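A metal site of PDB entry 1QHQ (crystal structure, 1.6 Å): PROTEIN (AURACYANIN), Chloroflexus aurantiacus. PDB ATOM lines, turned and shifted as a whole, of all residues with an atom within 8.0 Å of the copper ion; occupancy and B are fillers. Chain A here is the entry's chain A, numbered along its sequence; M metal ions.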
ATOM      1  N   ALA A  23       0.314   1.595 -31.948  1.00  0.00           N
ATOM      2  CA  ALA A  23      -0.828   2.529 -32.169  1.00  0.00           C
ATOM      3  C   ALA A  23      -1.818   1.881 -33.113  1.00  0.00           C
ATOM      4  O   ALA A  23      -1.458   1.001 -33.914  1.00  0.00           O
ATOM      5  CB  ALA A  23      -0.279   3.821 -32.759  1.00  0.00           C
ATOM      6  N   ALA A  27      -6.810   5.148 -36.168  1.00  0.00           N
ATOM      7  CA  ALA A  27      -7.611   5.741 -35.108  1.00  0.00           C
ATOM      8  C   ALA A  27      -6.748   6.351 -34.039  1.00  0.00           C
ATOM      9  O   ALA A  27      -5.575   5.918 -33.873  1.00  0.00           O
ATOM     10  CB  ALA A  27      -8.535   4.679 -34.482  1.00  0.00           C
ATOM     11  N   LEU A  28      -7.252   7.229 -33.213  1.00  0.00           N
ATOM     12  CA  LEU A  28      -6.577   7.741 -32.045  1.00  0.00           C
ATOM     13  C   LEU A  28      -6.777   6.787 -30.862  1.00  0.00           C
ATOM     14  O   LEU A  28      -7.566   6.976 -29.958  1.00  0.00           O
ATOM     15  CB  LEU A  28      -7.067   9.149 -31.711  1.00  0.00           C
ATOM     16  CG  LEU A  28      -6.998  10.129 -32.912  1.00  0.00           C
ATOM     17  CD1 LEU A  28      -7.509  11.496 -32.463  1.00  0.00           C
ATOM     18  CD2 LEU A  28      -5.590  10.235 -33.446  1.00  0.00           C
ATOM     19  N   ALA A  29      -6.034   5.666 -30.946  1.00  0.00           N
ATOM     20  CA  ALA A  29      -6.189   4.618 -29.927  1.00  0.00           C
ATOM     21  C   ALA A  29      -4.897   3.767 -29.926  1.00  0.00           C
ATOM     22  O   ALA A  29      -4.174   3.727 -30.905  1.00  0.00           O
ATOM     23  CB  ALA A  29      -7.339   3.706 -30.299  1.00  0.00           C
ATOM     24  N   PHE A  30      -4.728   3.068 -28.802  1.00  0.00           N
ATOM     25  CA  PHE A  30      -3.691   2.014 -28.798  1.00  0.00           C
ATOM     26  C   PHE A  30      -4.317   0.783 -29.445  1.00  0.00           C
ATOM     27  O   PHE A  30      -5.507   0.509 -29.261  1.00  0.00           O
ATOM     28  CB  PHE A  30      -3.333   1.702 -27.337  1.00  0.00           C
ATOM     29  CG  PHE A  30      -2.637   2.813 -26.638  1.00  0.00           C
ATOM     30  CD1 PHE A  30      -1.316   3.166 -26.950  1.00  0.00           C
ATOM     31  CD2 PHE A  30      -3.288   3.579 -25.661  1.00  0.00           C
ATOM     32  CE1 PHE A  30      -0.708   4.211 -26.332  1.00  0.00           C
ATOM     33  CE2 PHE A  30      -2.674   4.635 -25.051  1.00  0.00           C
ATOM     34  CZ  PHE A  30      -1.346   4.960 -25.359  1.00  0.00           C
ATOM     35  N   PHE A  47       7.029   1.096 -27.407  1.00  0.00           N
ATOM     36  CA  PHE A  47       5.837   1.635 -28.134  1.00  0.00           C
ATOM     37  C   PHE A  47       6.247   1.973 -29.571  1.00  0.00           C
ATOM     38  O   PHE A  47       7.176   2.733 -29.815  1.00  0.00           O
ATOM     39  CB  PHE A  47       5.431   2.931 -27.408  1.00  0.00           C
ATOM     40  CG  PHE A  47       4.197   3.593 -27.995  1.00  0.00           C
ATOM     41  CD1 PHE A  47       3.208   2.804 -28.529  1.00  0.00           C
ATOM     42  CD2 PHE A  47       4.089   4.961 -28.001  1.00  0.00           C
ATOM     43  CE1 PHE A  47       2.078   3.397 -29.128  1.00  0.00           C
ATOM     44  CE2 PHE A  47       2.959   5.537 -28.569  1.00  0.00           C
ATOM     45  CZ  PHE A  47       1.962   4.769 -29.093  1.00  0.00           C
ATOM     46  N   ASN A  49       5.011   3.479 -32.901  1.00  0.00           N
ATOM     47  CA  ASN A  49       3.967   4.351 -33.460  1.00  0.00           C
ATOM     48  C   ASN A  49       3.945   4.271 -34.992  1.00  0.00           C
ATOM     49  O   ASN A  49       4.553   5.158 -35.607  1.00  0.00           O
ATOM     50  CB  ASN A  49       4.164   5.787 -33.008  1.00  0.00           C
ATOM     51  CG  ASN A  49       2.963   6.682 -33.552  1.00  0.00           C
ATOM     52  OD1 ASN A  49       2.014   6.108 -33.969  1.00  0.00           O
ATOM     53  ND2 ASN A  49       3.193   7.953 -33.461  1.00  0.00           N
ATOM     54  N   ASN A  51       1.336   4.556 -38.013  1.00  0.00           N
ATOM     55  CA  ASN A  51      -0.088   4.884 -38.235  1.00  0.00           C
ATOM     56  C   ASN A  51      -0.231   5.590 -39.593  1.00  0.00           C
ATOM     57  O   ASN A  51       0.738   6.151 -40.079  1.00  0.00           O
ATOM     58  CB  ASN A  51      -0.656   5.724 -37.114  1.00  0.00           C
ATOM     59  CG  ASN A  51      -0.192   7.131 -37.002  1.00  0.00           C
ATOM     60  OD1 ASN A  51      -0.592   8.025 -37.787  1.00  0.00           O
ATOM     61  ND2 ASN A  51       0.642   7.471 -36.028  1.00  0.00           N
ATOM     62  N   VAL A  55       0.203  11.020 -37.364  1.00  0.00           N
ATOM     63  CA  VAL A  55      -0.003  11.613 -36.063  1.00  0.00           C
ATOM     64  C   VAL A  55       0.947  11.112 -34.979  1.00  0.00           C
ATOM     65  O   VAL A  55       1.450   9.985 -35.033  1.00  0.00           O
ATOM     66  CB  VAL A  55      -1.475  11.480 -35.604  1.00  0.00           C
ATOM     67  CG1 VAL A  55      -1.755  10.083 -35.079  1.00  0.00           C
ATOM     68  CG2 VAL A  55      -1.811  12.563 -34.593  1.00  0.00           C
ATOM     69  N   GLN A  56       1.270  11.978 -34.056  1.00  0.00           N
ATOM     70  CA  GLN A  56       2.100  11.706 -32.898  1.00  0.00           C
ATOM     71  C   GLN A  56       1.354  11.010 -31.770  1.00  0.00           C
ATOM     72  O   GLN A  56       0.184  11.256 -31.551  1.00  0.00           O
ATOM     73  CB  GLN A  56       2.659  13.020 -32.357  1.00  0.00           C
ATOM     74  CG  GLN A  56       3.660  13.657 -33.342  1.00  0.00           C
ATOM     75  CD  GLN A  56       3.858  15.120 -33.000  1.00  0.00           C
ATOM     76  OE1 GLN A  56       2.909  15.910 -33.195  1.00  0.00           O
ATOM     77  NE2 GLN A  56       4.993  15.476 -32.480  1.00  0.00           N
ATOM     78  N   HIS A  57       2.123  10.224 -30.972  1.00  0.00           N
ATOM     79  CA  HIS A  57       1.534   9.504 -29.857  1.00  0.00           C
ATOM     80  C   HIS A  57       2.646   9.142 -28.829  1.00  0.00           C
ATOM     81  O   HIS A  57       3.801   8.989 -29.167  1.00  0.00           O
ATOM     82  CB  HIS A  57       0.984   8.155 -30.293  1.00  0.00           C
ATOM     83  CG  HIS A  57      -0.202   8.108 -31.203  1.00  0.00           C
ATOM     84  ND1 HIS A  57      -1.415   8.673 -30.855  1.00  0.00           N
ATOM     85  CD2 HIS A  57      -0.404   7.422 -32.330  1.00  0.00           C
ATOM     86  CE1 HIS A  57      -2.293   8.390 -31.791  1.00  0.00           C
ATOM     87  NE2 HIS A  57      -1.718   7.632 -32.716  1.00  0.00           N
ATOM     88  N   ASN A  58       2.158   9.028 -27.585  1.00  0.00           N
ATOM     89  CA  ASN A  58       3.093   8.518 -26.538  1.00  0.00           C
ATOM     90  C   ASN A  58       2.285   7.501 -25.730  1.00  0.00           C
ATOM     91  O   ASN A  58       1.170   7.174 -25.997  1.00  0.00           O
ATOM     92  CB  ASN A  58       3.705   9.563 -25.697  1.00  0.00           C
ATOM     93  CG  ASN A  58       2.820  10.298 -24.737  1.00  0.00           C
ATOM     94  OD1 ASN A  58       1.590  10.109 -24.842  1.00  0.00           O
ATOM     95  ND2 ASN A  58       3.353  11.091 -23.836  1.00  0.00           N
ATOM     96  N   TRP A  59       3.019   6.849 -24.800  1.00  0.00           N
ATOM     97  CA  TRP A  59       2.404   5.891 -23.855  1.00  0.00           C
ATOM     98  C   TRP A  59       2.740   6.377 -22.456  1.00  0.00           C
ATOM     99  O   TRP A  59       3.946   6.580 -22.126  1.00  0.00           O
ATOM    100  CB  TRP A  59       2.906   4.497 -24.101  1.00  0.00           C
ATOM    101  CG  TRP A  59       2.331   3.440 -23.191  1.00  0.00           C
ATOM    102  CD1 TRP A  59       1.229   2.699 -23.462  1.00  0.00           C
ATOM    103  CD2 TRP A  59       2.828   3.002 -21.925  1.00  0.00           C
ATOM    104  NE1 TRP A  59       0.994   1.790 -22.419  1.00  0.00           N
ATOM    105  CE2 TRP A  59       1.967   2.017 -21.468  1.00  0.00           C
ATOM    106  CE3 TRP A  59       3.925   3.383 -21.147  1.00  0.00           C
ATOM    107  CZ2 TRP A  59       2.182   1.320 -20.264  1.00  0.00           C
ATOM    108  CZ3 TRP A  59       4.141   2.721 -19.917  1.00  0.00           C
ATOM    109  CH2 TRP A  59       3.254   1.746 -19.495  1.00  0.00           C
ATOM    110  N   MET A  99       7.318  11.440 -26.926  1.00  0.00           N
ATOM    111  CA  MET A  99       6.232  11.607 -27.911  1.00  0.00           C
ATOM    112  C   MET A  99       6.808  11.275 -29.300  1.00  0.00           C
ATOM    113  O   MET A  99       7.849  11.831 -29.658  1.00  0.00           O
ATOM    114  CB  MET A  99       5.787  13.075 -27.841  1.00  0.00           C
ATOM    115  CG  MET A  99       4.565  13.333 -28.735  1.00  0.00           C
ATOM    116  SD  MET A  99       3.116  12.423 -28.208  1.00  0.00           S
ATOM    117  CE  MET A  99       2.719  13.197 -26.668  1.00  0.00           C
ATOM    118  N   LEU A 100       6.212  10.312 -29.952  1.00  0.00           N
ATOM    119  CA  LEU A 100       6.767   9.711 -31.140  1.00  0.00           C
ATOM    120  C   LEU A 100       6.049  10.174 -32.411  1.00  0.00           C
ATOM    121  O   LEU A 100       4.823  10.129 -32.464  1.00  0.00           O
ATOM    122  CB  LEU A 100       6.560   8.157 -31.057  1.00  0.00           C
ATOM    123  CG  LEU A 100       7.185   7.568 -29.770  1.00  0.00           C
ATOM    124  CD1 LEU A 100       6.864   6.086 -29.706  1.00  0.00           C
ATOM    125  CD2 LEU A 100       8.695   7.785 -29.755  1.00  0.00           C
ATOM    126  N   ILE A 121      -2.426   6.101 -20.895  1.00  0.00           N
ATOM    127  CA  ILE A 121      -3.069   7.023 -21.849  1.00  0.00           C
ATOM    128  C   ILE A 121      -2.008   7.556 -22.792  1.00  0.00           C
ATOM    129  O   ILE A 121      -0.802   7.416 -22.603  1.00  0.00           O
ATOM    130  CB  ILE A 121      -3.696   8.261 -21.127  1.00  0.00           C
ATOM    131  CG1 ILE A 121      -2.642   9.087 -20.447  1.00  0.00           C
ATOM    132  CG2 ILE A 121      -4.763   7.776 -20.131  1.00  0.00           C
ATOM    133  CD1 ILE A 121      -3.169  10.316 -19.678  1.00  0.00           C
ATOM    134  N   CYS A 122      -2.479   8.274 -23.812  1.00  0.00           N
ATOM    135  CA  CYS A 122      -1.607   9.075 -24.647  1.00  0.00           C
ATOM    136  C   CYS A 122      -1.881  10.549 -24.245  1.00  0.00           C
ATOM    137  O   CYS A 122      -3.069  10.871 -24.050  1.00  0.00           O
ATOM    138  CB  CYS A 122      -1.890   8.854 -26.104  1.00  0.00           C
ATOM    139  SG  CYS A 122      -1.016  10.027 -27.196  1.00  0.00           S
ATOM    140  N   THR A 123      -0.867  11.346 -24.081  1.00  0.00           N
ATOM    141  CA  THR A 123      -1.063  12.734 -23.694  1.00  0.00           C
ATOM    142  C   THR A 123      -0.974  13.725 -24.850  1.00  0.00           C
ATOM    143  O   THR A 123      -1.084  14.927 -24.538  1.00  0.00           O
ATOM    144  CB  THR A 123      -0.141  13.180 -22.563  1.00  0.00           C
ATOM    145  OG1 THR A 123       1.230  13.014 -22.884  1.00  0.00           O
ATOM    146  CG2 THR A 123      -0.507  12.382 -21.301  1.00  0.00           C
ATOM    147  N   PHE A 124      -0.869  13.262 -26.072  1.00  0.00           N
ATOM    148  CA  PHE A 124      -0.899  14.303 -27.174  1.00  0.00           C
ATOM    149  C   PHE A 124      -2.277  14.966 -27.094  1.00  0.00           C
ATOM    150  O   PHE A 124      -3.266  14.287 -26.896  1.00  0.00           O
ATOM    151  CB  PHE A 124      -0.741  13.579 -28.500  1.00  0.00           C
ATOM    152  CG  PHE A 124      -0.421  14.621 -29.569  1.00  0.00           C
ATOM    153  CD1 PHE A 124       0.845  15.144 -29.683  1.00  0.00           C
ATOM    154  CD2 PHE A 124      -1.480  15.141 -30.307  1.00  0.00           C
ATOM    155  CE1 PHE A 124       1.100  16.135 -30.615  1.00  0.00           C
ATOM    156  CE2 PHE A 124      -1.224  16.146 -31.219  1.00  0.00           C
ATOM    157  CZ  PHE A 124       0.053  16.646 -31.371  1.00  0.00           C
ATOM    158  N   PRO A 125      -2.313  16.287 -27.199  1.00  0.00           N
ATOM    159  CA  PRO A 125      -3.566  17.031 -27.068  1.00  0.00           C
ATOM    160  C   PRO A 125      -4.741  16.403 -27.751  1.00  0.00           C
ATOM    161  O   PRO A 125      -4.728  16.059 -28.921  1.00  0.00           O
ATOM    162  CB  PRO A 125      -3.227  18.387 -27.708  1.00  0.00           C
ATOM    163  CG  PRO A 125      -1.779  18.547 -27.469  1.00  0.00           C
ATOM    164  CD  PRO A 125      -1.177  17.152 -27.532  1.00  0.00           C
ATOM    165  N   GLY A 126      -5.838  16.184 -26.958  1.00  0.00           N
ATOM    166  CA  GLY A 126      -7.021  15.584 -27.494  1.00  0.00           C
ATOM    167  C   GLY A 126      -7.145  14.102 -27.503  1.00  0.00           C
ATOM    168  O   GLY A 126      -8.241  13.533 -27.594  1.00  0.00           O
ATOM    169  N   HIS A 127      -6.011  13.343 -27.509  1.00  0.00           N
ATOM    170  CA  HIS A 127      -6.097  11.912 -27.675  1.00  0.00           C
ATOM    171  C   HIS A 127      -6.719  11.193 -26.487  1.00  0.00           C
ATOM    172  O   HIS A 127      -7.534  10.296 -26.693  1.00  0.00           O
ATOM    173  CB  HIS A 127      -4.660  11.375 -27.936  1.00  0.00           C
ATOM    174  CG  HIS A 127      -4.191  11.789 -29.312  1.00  0.00           C
ATOM    175  ND1 HIS A 127      -3.098  11.156 -29.920  1.00  0.00           N
ATOM    176  CD2 HIS A 127      -4.627  12.688 -30.212  1.00  0.00           C
ATOM    177  CE1 HIS A 127      -2.935  11.656 -31.148  1.00  0.00           C
ATOM    178  NE2 HIS A 127      -3.837  12.555 -31.323  1.00  0.00           N
ATOM    179  N   TYR A 128      -6.387  11.642 -25.287  1.00  0.00           N
ATOM    180  CA  TYR A 128      -6.980  11.017 -24.073  1.00  0.00           C
ATOM    181  C   TYR A 128      -8.486  11.226 -24.025  1.00  0.00           C
ATOM    182  O   TYR A 128      -9.243  10.261 -23.999  1.00  0.00           O
ATOM    183  CB  TYR A 128      -6.287  11.585 -22.835  1.00  0.00           C
ATOM    184  CG  TYR A 128      -6.989  11.173 -21.537  1.00  0.00           C
ATOM    185  CD1 TYR A 128      -7.250   9.849 -21.276  1.00  0.00           C
ATOM    186  CD2 TYR A 128      -7.515  12.151 -20.702  1.00  0.00           C
ATOM    187  CE1 TYR A 128      -7.998   9.461 -20.168  1.00  0.00           C
ATOM    188  CE2 TYR A 128      -8.276  11.782 -19.592  1.00  0.00           C
ATOM    189  CZ  TYR A 128      -8.449  10.451 -19.314  1.00  0.00           C
ATOM    190  OH  TYR A 128      -9.242  10.080 -18.230  1.00  0.00           O
ATOM    191  N   MET A 132      -8.035   7.493 -26.274  1.00  0.00           N
ATOM    192  CA  MET A 132      -6.736   6.792 -26.400  1.00  0.00           C
ATOM    193  C   MET A 132      -6.202   6.488 -24.989  1.00  0.00           C
ATOM    194  O   MET A 132      -5.474   7.249 -24.389  1.00  0.00           O
ATOM    195  CB  MET A 132      -5.717   7.619 -27.169  1.00  0.00           C
ATOM    196  CG  MET A 132      -4.432   6.729 -27.439  1.00  0.00           C
ATOM    197  SD  MET A 132      -3.582   7.417 -28.901  1.00  0.00           S
ATOM    198  CE  MET A 132      -2.146   6.260 -28.890  1.00  0.00           C
ATOM    199  N   LYS A 133      -6.623   5.301 -24.559  1.00  0.00           N
ATOM    200  CA  LYS A 133      -6.280   4.870 -23.176  1.00  0.00           C
ATOM    201  C   LYS A 133      -6.386   3.342 -23.171  1.00  0.00           C
ATOM    202  O   LYS A 133      -6.986   2.775 -24.047  1.00  0.00           O
ATOM    203  CB  LYS A 133      -7.215   5.480 -22.192  1.00  0.00           C
ATOM    204  CG  LYS A 133      -8.692   5.113 -22.296  1.00  0.00           C
ATOM    205  CD  LYS A 133      -9.429   5.876 -21.183  1.00  0.00           C
ATOM    206  CE  LYS A 133     -10.921   5.988 -21.491  1.00  0.00           C
ATOM    207  NZ  LYS A 133     -11.505   7.054 -20.580  1.00  0.00           N
HETATM  208 CU    CU M   1      -1.901   9.693 -29.180  1.00  0.00          CU
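Residues that only touch the copper ion: Gln 56 (3.5 Å). Five residues have an atom within 4 Å of the copper ion: Gln 56, His 57, Cys 122, His 127 and Met 132. The nearest printed residue that does not touch the copper ion is Phe 124 (4.1 Å).
The copper ion is bound by a ring nitrogen (ND1) of His 57, 2.0 Å away. The copper ion is bound by ND1 of His 127, 2.0 Å away. The copper ion is bound by SG of Cys 122, 2.2 Å away. The copper ion has three donor atoms within binding distance. Slightly farther from the copper ion lies the side-chain sulfur (SD) of Met 132 (2.8 Å).
The side-chain sulfur of Met 99 sits close to the backbone NH of His 57 (3.7 Å). The backbone carbonyl oxygen (O) of His 57 lies within hydrogen-bond range of the backbone NH (N) of Leu 100 (2.9 Å). N of Cys 122 sits at hydrogen-bond distance from O of Met 132 (3.2 Å). SD of Met 132 lies within hydrogen-bond range of N of Ala 29, 3.6 Å away. The backbone carbonyl oxygen (O) of His 127 sits at hydrogen-bond distance from the backbone NH (N) of Met 132 (2.9 Å). The side-chain sulfur (SG) of Cys 122 sits close to the backbone NH (N) of Asn 58, at 3.4 Å. SG of Cys 122 sits close to N of Phe 124. A ring nitrogen (ND1) of His 57 lies close to the side-chain sulfur (SD) of Met 132, at 3.2 Å.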
